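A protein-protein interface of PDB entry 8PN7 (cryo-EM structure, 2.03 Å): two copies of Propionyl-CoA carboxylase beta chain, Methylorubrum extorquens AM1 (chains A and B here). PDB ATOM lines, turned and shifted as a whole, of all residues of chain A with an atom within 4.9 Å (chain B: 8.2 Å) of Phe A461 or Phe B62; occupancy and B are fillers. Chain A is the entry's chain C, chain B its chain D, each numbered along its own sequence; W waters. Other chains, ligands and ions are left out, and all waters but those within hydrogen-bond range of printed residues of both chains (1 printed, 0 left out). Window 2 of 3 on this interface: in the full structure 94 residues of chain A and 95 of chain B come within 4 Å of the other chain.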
ATOM      1  N   ILE A 427      -1.349  -9.875  20.583  1.00  0.00           N
ATOM      2  CA  ILE A 427      -0.174 -10.723  20.741  1.00  0.00           C
ATOM      3  C   ILE A 427       1.027  -9.809  20.946  1.00  0.00           C
ATOM      4  O   ILE A 427       1.469  -9.131  20.013  1.00  0.00           O
ATOM      5  CB  ILE A 427       0.016 -11.647  19.532  1.00  0.00           C
ATOM      6  CG1 ILE A 427      -1.309 -12.325  19.180  1.00  0.00           C
ATOM      7  CG2 ILE A 427       1.086 -12.687  19.815  1.00  0.00           C
ATOM      8  CD1 ILE A 427      -1.287 -13.073  17.872  1.00  0.00           C
ATOM      9  N   ALA A 428       1.556  -9.789  22.165  1.00  0.00           N
ATOM     10  CA  ALA A 428       2.640  -8.883  22.512  1.00  0.00           C
ATOM     11  C   ALA A 428       3.439  -9.475  23.664  1.00  0.00           C
ATOM     12  O   ALA A 428       3.009 -10.424  24.324  1.00  0.00           O
ATOM     13  CB  ALA A 428       2.108  -7.492  22.874  1.00  0.00           C
ATOM     14  N   ILE A 439      10.929   0.349  28.144  1.00  0.00           N
ATOM     15  CA  ILE A 439      11.665   0.862  26.991  1.00  0.00           C
ATOM     16  C   ILE A 439      12.087   2.309  27.219  1.00  0.00           C
ATOM     17  O   ILE A 439      13.188   2.718  26.833  1.00  0.00           O
ATOM     18  CB  ILE A 439      10.821   0.708  25.712  1.00  0.00           C
ATOM     19  CG1 ILE A 439      10.603  -0.771  25.394  1.00  0.00           C
ATOM     20  CG2 ILE A 439      11.483   1.411  24.538  1.00  0.00           C
ATOM     21  CD1 ILE A 439       9.677  -1.015  24.225  1.00  0.00           C
ATOM     22  N   PHE A 440      11.231   3.100  27.858  1.00  0.00           N
ATOM     23  CA  PHE A 440      11.472   4.520  28.083  1.00  0.00           C
ATOM     24  C   PHE A 440      11.658   4.814  29.568  1.00  0.00           C
ATOM     25  O   PHE A 440      11.102   5.774  30.106  1.00  0.00           O
ATOM     26  CB  PHE A 440      10.337   5.359  27.504  1.00  0.00           C
ATOM     27  CG  PHE A 440      10.090   5.113  26.043  1.00  0.00           C
ATOM     28  CD1 PHE A 440      10.897   5.697  25.083  1.00  0.00           C
ATOM     29  CD2 PHE A 440       9.048   4.299  25.631  1.00  0.00           C
ATOM     30  CE1 PHE A 440      10.672   5.473  23.740  1.00  0.00           C
ATOM     31  CE2 PHE A 440       8.819   4.072  24.290  1.00  0.00           C
ATOM     32  CZ  PHE A 440       9.631   4.660  23.344  1.00  0.00           C
ATOM     33  N   TYR A 457       2.447   2.735  21.345  1.00  0.00           N
ATOM     34  CA  TYR A 457       2.746   1.316  21.503  1.00  0.00           C
ATOM     35  C   TYR A 457       1.485   0.472  21.376  1.00  0.00           C
ATOM     36  O   TYR A 457       1.505  -0.598  20.756  1.00  0.00           O
ATOM     37  CB  TYR A 457       3.426   1.070  22.850  1.00  0.00           C
ATOM     38  CG  TYR A 457       4.118  -0.271  22.947  1.00  0.00           C
ATOM     39  CD1 TYR A 457       3.419  -1.411  23.321  1.00  0.00           C
ATOM     40  CD2 TYR A 457       5.471  -0.397  22.663  1.00  0.00           C
ATOM     41  CE1 TYR A 457       4.046  -2.637  23.408  1.00  0.00           C
ATOM     42  CE2 TYR A 457       6.106  -1.620  22.748  1.00  0.00           C
ATOM     43  CZ  TYR A 457       5.389  -2.736  23.120  1.00  0.00           C
ATOM     44  OH  TYR A 457       6.017  -3.955  23.206  1.00  0.00           O
ATOM     45  N   GLU A 458       0.377   0.936  21.958  1.00  0.00           N
ATOM     46  CA  GLU A 458      -0.888   0.220  21.836  1.00  0.00           C
ATOM     47  C   GLU A 458      -1.326   0.124  20.382  1.00  0.00           C
ATOM     48  O   GLU A 458      -1.804  -0.926  19.937  1.00  0.00           O
ATOM     49  CB  GLU A 458      -1.959   0.918  22.675  1.00  0.00           C
ATOM     50  CG  GLU A 458      -2.545   0.070  23.788  1.00  0.00           C
ATOM     51  CD  GLU A 458      -3.599  -0.901  23.293  1.00  0.00           C
ATOM     52  OE1 GLU A 458      -3.940  -0.852  22.093  1.00  0.00           O
ATOM     53  OE2 GLU A 458      -4.090  -1.711  24.107  1.00  0.00           O
ATOM     54  N   ASP A 459      -1.174   1.213  19.626  1.00  0.00           N
ATOM     55  CA  ASP A 459      -1.549   1.189  18.215  1.00  0.00           C
ATOM     56  C   ASP A 459      -0.643   0.264  17.410  1.00  0.00           C
ATOM     57  O   ASP A 459      -1.107  -0.418  16.489  1.00  0.00           O
ATOM     58  CB  ASP A 459      -1.518   2.604  17.639  1.00  0.00           C
ATOM     59  CG  ASP A 459      -2.572   3.504  18.251  1.00  0.00           C
ATOM     60  OD1 ASP A 459      -3.314   3.037  19.141  1.00  0.00           O
ATOM     61  OD2 ASP A 459      -2.659   4.680  17.840  1.00  0.00           O
ATOM     62  N   ARG A 460       0.650   0.228  17.735  1.00  0.00           N
ATOM     63  CA  ARG A 460       1.588  -0.519  16.902  1.00  0.00           C
ATOM     64  C   ARG A 460       1.585  -2.014  17.206  1.00  0.00           C
ATOM     65  O   ARG A 460       1.597  -2.831  16.280  1.00  0.00           O
ATOM     66  CB  ARG A 460       3.003   0.037  17.067  1.00  0.00           C
ATOM     67  CG  ARG A 460       3.221   1.401  16.443  1.00  0.00           C
ATOM     68  CD  ARG A 460       4.691   1.778  16.484  1.00  0.00           C
ATOM     69  NE  ARG A 460       5.509   0.842  15.723  1.00  0.00           N
ATOM     70  CZ  ARG A 460       6.835   0.832  15.723  1.00  0.00           C
ATOM     71  NH1 ARG A 460       7.533   1.687  16.451  1.00  0.00           N
ATOM     72  NH2 ARG A 460       7.476  -0.062  14.975  1.00  0.00           N
ATOM     73  N   PHE A 461       1.569  -2.397  18.484  1.00  0.00           N
ATOM     74  CA  PHE A 461       1.894  -3.765  18.860  1.00  0.00           C
ATOM     75  C   PHE A 461       0.774  -4.538  19.542  1.00  0.00           C
ATOM     76  O   PHE A 461       0.834  -5.771  19.560  1.00  0.00           O
ATOM     77  CB  PHE A 461       3.129  -3.782  19.774  1.00  0.00           C
ATOM     78  CG  PHE A 461       4.327  -3.101  19.179  1.00  0.00           C
ATOM     79  CD1 PHE A 461       5.066  -3.717  18.184  1.00  0.00           C
ATOM     80  CD2 PHE A 461       4.709  -1.842  19.605  1.00  0.00           C
ATOM     81  CE1 PHE A 461       6.165  -3.092  17.630  1.00  0.00           C
ATOM     82  CE2 PHE A 461       5.807  -1.213  19.056  1.00  0.00           C
ATOM     83  CZ  PHE A 461       6.536  -1.838  18.067  1.00  0.00           C
ATOM     84  N   LEU A 462      -0.238  -3.871  20.094  1.00  0.00           N
ATOM     85  CA  LEU A 462      -1.332  -4.576  20.767  1.00  0.00           C
ATOM     86  C   LEU A 462      -2.394  -4.962  19.736  1.00  0.00           C
ATOM     87  O   LEU A 462      -3.528  -4.481  19.731  1.00  0.00           O
ATOM     88  CB  LEU A 462      -1.907  -3.725  21.893  1.00  0.00           C
ATOM     89  CG  LEU A 462      -1.251  -3.893  23.268  1.00  0.00           C
ATOM     90  CD1 LEU A 462      -1.357  -5.332  23.744  1.00  0.00           C
ATOM     91  CD2 LEU A 462       0.202  -3.447  23.258  1.00  0.00           C
ATOM     92  N   SER A 463      -1.992  -5.871  18.857  1.00  0.00           N
ATOM     93  CA  SER A 463      -2.804  -6.289  17.723  1.00  0.00           C
ATOM     94  C   SER A 463      -2.273  -7.631  17.240  1.00  0.00           C
ATOM     95  O   SER A 463      -1.176  -8.050  17.634  1.00  0.00           O
ATOM     96  CB  SER A 463      -2.766  -5.240  16.597  1.00  0.00           C
ATOM     97  OG  SER A 463      -1.471  -5.151  16.030  1.00  0.00           O
ATOM     98  N   VAL A 466       1.414  -7.756  13.980  1.00  0.00           N
ATOM     99  CA  VAL A 466       2.858  -7.975  14.018  1.00  0.00           C
ATOM    100  C   VAL A 466       3.169  -9.463  13.900  1.00  0.00           C
ATOM    101  O   VAL A 466       4.061  -9.871  13.145  1.00  0.00           O
ATOM    102  CB  VAL A 466       3.464  -7.366  15.294  1.00  0.00           C
ATOM    103  CG1 VAL A 466       4.953  -7.660  15.365  1.00  0.00           C
ATOM    104  CG2 VAL A 466       3.213  -5.869  15.336  1.00  0.00           C
ATOM    105  N   SER B  59      17.153  -5.800  14.729  1.00  0.00           N
ATOM    106  CA  SER B  59      16.016  -5.003  15.165  1.00  0.00           C
ATOM    107  C   SER B  59      16.246  -3.527  14.870  1.00  0.00           C
ATOM    108  O   SER B  59      17.341  -2.998  15.080  1.00  0.00           O
ATOM    109  CB  SER B  59      15.766  -5.205  16.659  1.00  0.00           C
ATOM    110  OG  SER B  59      14.676  -4.417  17.105  1.00  0.00           O
ATOM    111  N   THR B  60      15.201  -2.862  14.378  1.00  0.00           N
ATOM    112  CA  THR B  60      15.250  -1.433  14.085  1.00  0.00           C
ATOM    113  C   THR B  60      14.239  -0.635  14.897  1.00  0.00           C
ATOM    114  O   THR B  60      14.007   0.541  14.594  1.00  0.00           O
ATOM    115  CB  THR B  60      15.027  -1.183  12.590  1.00  0.00           C
ATOM    116  OG1 THR B  60      13.782  -1.768  12.184  1.00  0.00           O
ATOM    117  CG2 THR B  60      16.158  -1.787  11.771  1.00  0.00           C
ATOM    118  N   ASP B  61      13.633  -1.235  15.917  1.00  0.00           N
ATOM    119  CA  ASP B  61      12.639  -0.554  16.734  1.00  0.00           C
ATOM    120  C   ASP B  61      13.288   0.087  17.952  1.00  0.00           C
ATOM    121  O   ASP B  61      14.204  -0.480  18.554  1.00  0.00           O
ATOM    122  CB  ASP B  61      11.548  -1.529  17.178  1.00  0.00           C
ATOM    123  CG  ASP B  61      10.670  -1.982  16.030  1.00  0.00           C
ATOM    124  OD1 ASP B  61      10.478  -1.194  15.081  1.00  0.00           O
ATOM    125  OD2 ASP B  61      10.170  -3.125  16.078  1.00  0.00           O
ATOM    126  N   PHE B  62      12.804   1.278  18.305  1.00  0.00           N
ATOM    127  CA  PHE B  62      13.228   1.992  19.512  1.00  0.00           C
ATOM    128  C   PHE B  62      14.731   2.258  19.515  1.00  0.00           C
ATOM    129  O   PHE B  62      15.387   2.208  20.556  1.00  0.00           O
ATOM    130  CB  PHE B  62      12.809   1.234  20.773  1.00  0.00           C
ATOM    131  CG  PHE B  62      11.361   0.847  20.788  1.00  0.00           C
ATOM    132  CD1 PHE B  62      10.383   1.785  21.067  1.00  0.00           C
ATOM    133  CD2 PHE B  62      10.975  -0.455  20.520  1.00  0.00           C
ATOM    134  CE1 PHE B  62       9.050   1.434  21.079  1.00  0.00           C
ATOM    135  CE2 PHE B  62       9.642  -0.811  20.530  1.00  0.00           C
ATOM    136  CZ  PHE B  62       8.679   0.134  20.810  1.00  0.00           C
ATOM    137  N   GLY B  63      15.282   2.543  18.338  1.00  0.00           N
ATOM    138  CA  GLY B  63      16.686   2.886  18.242  1.00  0.00           C
ATOM    139  C   GLY B  63      17.648   1.745  18.476  1.00  0.00           C
ATOM    140  O   GLY B  63      18.817   1.991  18.779  1.00  0.00           O
ATOM    141  N   MET B  64      17.191   0.497  18.347  1.00  0.00           N
ATOM    142  CA  MET B  64      18.084  -0.640  18.533  1.00  0.00           C
ATOM    143  C   MET B  64      19.127  -0.748  17.430  1.00  0.00           C
ATOM    144  O   MET B  64      20.170  -1.375  17.642  1.00  0.00           O
ATOM    145  CB  MET B  64      17.281  -1.939  18.615  1.00  0.00           C
ATOM    146  CG  MET B  64      16.574  -2.143  19.940  1.00  0.00           C
ATOM    147  SD  MET B  64      17.719  -2.360  21.313  1.00  0.00           S
ATOM    148  CE  MET B  64      18.518  -3.891  20.838  1.00  0.00           C
ATOM    149  N   GLU B  65      18.876  -0.149  16.266  1.00  0.00           N
ATOM    150  CA  GLU B  65      19.834  -0.195  15.170  1.00  0.00           C
ATOM    151  C   GLU B  65      21.133   0.532  15.490  1.00  0.00           C
ATOM    152  O   GLU B  65      22.123   0.335  14.778  1.00  0.00           O
ATOM    153  CB  GLU B  65      19.214   0.395  13.899  1.00  0.00           C
ATOM    154  CG  GLU B  65      18.972   1.898  13.952  1.00  0.00           C
ATOM    155  CD  GLU B  65      17.763   2.278  14.789  1.00  0.00           C
ATOM    156  OE1 GLU B  65      16.946   1.386  15.102  1.00  0.00           O
ATOM    157  OE2 GLU B  65      17.631   3.469  15.133  1.00  0.00           O
ATOM    158  N   LYS B  66      21.155   1.358  16.535  1.00  0.00           N
ATOM    159  CA  LYS B  66      22.363   2.058  16.944  1.00  0.00           C
ATOM    160  C   LYS B  66      23.184   1.286  17.970  1.00  0.00           C
ATOM    161  O   LYS B  66      24.288   1.724  18.311  1.00  0.00           O
ATOM    162  CB  LYS B  66      22.005   3.439  17.505  1.00  0.00           C
ATOM    163  CG  LYS B  66      21.532   4.426  16.447  1.00  0.00           C
ATOM    164  CD  LYS B  66      20.317   5.213  16.914  1.00  0.00           C
ATOM    165  CE  LYS B  66      20.603   5.983  18.190  1.00  0.00           C
ATOM    166  NZ  LYS B  66      19.408   6.745  18.649  1.00  0.00           N
ATOM    167  N   GLN B  67      22.682   0.157  18.463  1.00  0.00           N
ATOM    168  CA  GLN B  67      23.401  -0.693  19.410  1.00  0.00           C
ATOM    169  C   GLN B  67      23.471  -2.098  18.822  1.00  0.00           C
ATOM    170  O   GLN B  67      22.617  -2.944  19.097  1.00  0.00           O
ATOM    171  CB  GLN B  67      22.728  -0.697  20.787  1.00  0.00           C
ATOM    172  CG  GLN B  67      22.932   0.574  21.594  1.00  0.00           C
ATOM    173  CD  GLN B  67      22.046   1.712  21.134  1.00  0.00           C
ATOM    174  OE1 GLN B  67      20.968   1.490  20.582  1.00  0.00           O
ATOM    175  NE2 GLN B  67      22.496   2.941  21.358  1.00  0.00           N
ATOM    176  N   ILE B 133      12.698  -6.749  25.261  1.00  0.00           N
ATOM    177  CA  ILE B 133      11.425  -6.046  25.127  1.00  0.00           C
ATOM    178  C   ILE B 133      11.360  -5.278  23.811  1.00  0.00           C
ATOM    179  O   ILE B 133      10.300  -5.196  23.179  1.00  0.00           O
ATOM    180  CB  ILE B 133      11.196  -5.125  26.343  1.00  0.00           C
ATOM    181  CG1 ILE B 133       9.915  -4.305  26.172  1.00  0.00           C
ATOM    182  CG2 ILE B 133      12.397  -4.220  26.575  1.00  0.00           C
ATOM    183  CD1 ILE B 133       8.662  -5.141  26.058  1.00  0.00           C
ATOM    184  N   GLN B 134      12.485  -4.710  23.372  1.00  0.00           N
ATOM    185  CA  GLN B 134      12.483  -3.887  22.168  1.00  0.00           C
ATOM    186  C   GLN B 134      12.173  -4.680  20.904  1.00  0.00           C
ATOM    187  O   GLN B 134      11.753  -4.084  19.909  1.00  0.00           O
ATOM    188  CB  GLN B 134      13.829  -3.177  22.008  1.00  0.00           C
ATOM    189  CG  GLN B 134      14.109  -2.103  23.045  1.00  0.00           C
ATOM    190  CD  GLN B 134      14.688  -2.660  24.329  1.00  0.00           C
ATOM    191  OE1 GLN B 134      14.896  -3.865  24.462  1.00  0.00           O
ATOM    192  NE2 GLN B 134      14.958  -1.779  25.284  1.00  0.00           N
ATOM    193  N   GLU B 135      12.368  -5.998  20.912  1.00  0.00           N
ATOM    194  CA  GLU B 135      12.170  -6.796  19.708  1.00  0.00           C
ATOM    195  C   GLU B 135      10.773  -7.390  19.587  1.00  0.00           C
ATOM    196  O   GLU B 135      10.472  -8.009  18.562  1.00  0.00           O
ATOM    197  CB  GLU B 135      13.206  -7.922  19.640  1.00  0.00           C
ATOM    198  CG  GLU B 135      14.624  -7.430  19.419  1.00  0.00           C
ATOM    199  CD  GLU B 135      15.485  -8.440  18.689  1.00  0.00           C
ATOM    200  OE1 GLU B 135      14.983  -9.542  18.380  1.00  0.00           O
ATOM    201  OE2 GLU B 135      16.664  -8.133  18.420  1.00  0.00           O
ATOM    202  N   GLY B 136       9.916  -7.216  20.590  1.00  0.00           N
ATOM    203  CA  GLY B 136       8.544  -7.683  20.467  1.00  0.00           C
ATOM    204  C   GLY B 136       8.438  -9.196  20.409  1.00  0.00           C
ATOM    205  O   GLY B 136       9.200  -9.927  21.050  1.00  0.00           O
ATOM    206  N   VAL B 137       7.475  -9.677  19.617  1.00  0.00           N
ATOM    207  CA  VAL B 137       7.127 -11.095  19.592  1.00  0.00           C
ATOM    208  C   VAL B 137       8.177 -11.973  18.927  1.00  0.00           C
ATOM    209  O   VAL B 137       8.092 -13.202  19.031  1.00  0.00           O
ATOM    210  CB  VAL B 137       5.766 -11.295  18.895  1.00  0.00           C
ATOM    211  CG1 VAL B 137       4.656 -10.663  19.717  1.00  0.00           C
ATOM    212  CG2 VAL B 137       5.794 -10.710  17.493  1.00  0.00           C
HETATM  213  O   HOH W   1      10.767   2.536  17.014  1.00  0.00           O
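The side-chain carboxylate (OD1) of Asp B61 is in salt-bridge range of the guanidinium group (NH2) of Arg A460, 3.2 Å away.
The backbone NH of Ile A427 lies within hydrogen-bond range of the backbone carbonyl oxygen of Ser A463.
Among the printed residues, pairs that only touch across the chains: Ile A427 with Val B137 (3.5 Å), Ala A428 with Val B137 (3.9 Å), Ile A439 with Phe B62 (3.7 Å), Ile A439 with Ile B133 (3.7 Å), Phe A440 with Phe B62 (3.7 Å), Tyr A457 with Phe B62 (3.7 Å), Phe A461 with Phe B62 (3.6 Å) and Val A466 with Val B137 (3.8 Å).
Of the printed residues of chain B, Ile A439 touches Phe B62 (3.7 Å) and Ile B133 (3.7 Å). Of the printed residues of chain B, Tyr A457 touches Phe B62 (3.7 Å). Phe A461 touches one residue of chain B. Of the printed residues of chain B, Val A466 touches Val B137. Of chain A, only Ile A439 (3.7 Å), Phe A440 (3.7 Å), Tyr A457 (3.7 Å) and Phe A461 (3.6 Å) come within 4 Å of Phe B62. Of the printed residues of chain A, Val B137 touches Ile A427, Ala A428 and Val A466. The nearest printed residue of chain A that does not touch Asp B61 is Phe A461 (4.3 Å).
Of the 12 printed residues of chain A, 8 touch a printed residue of chain B. Hydrophobic or aromatic side chains of chain A that line the printed part of chain B: Ile A439, Phe A440, Tyr A457, Phe A461 and Val A466. Hydrophobic or aromatic side chains of chain B within 4 Å of the printed part of chain A: Phe B62, Ile B133 and Val B137. Among the printed residues, 9 pairs touch across the chains. Among the printed residues, Asp or Glu carboxylates within 4 Å of a Lys or Arg side-chain nitrogen of the other chain: Arg A460 with Asp B61 (3.2 Å).
No position is printed for both chains. Of the 9 pairs that touch across the chains among the printed residues, none has its exchanged pair printed and touching as well.
Water W1 bridges the backbone NH (N) of Phe B62 (2.7 Å) and the guanidinium group (NH1) of Arg A460 (3.4 Å).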
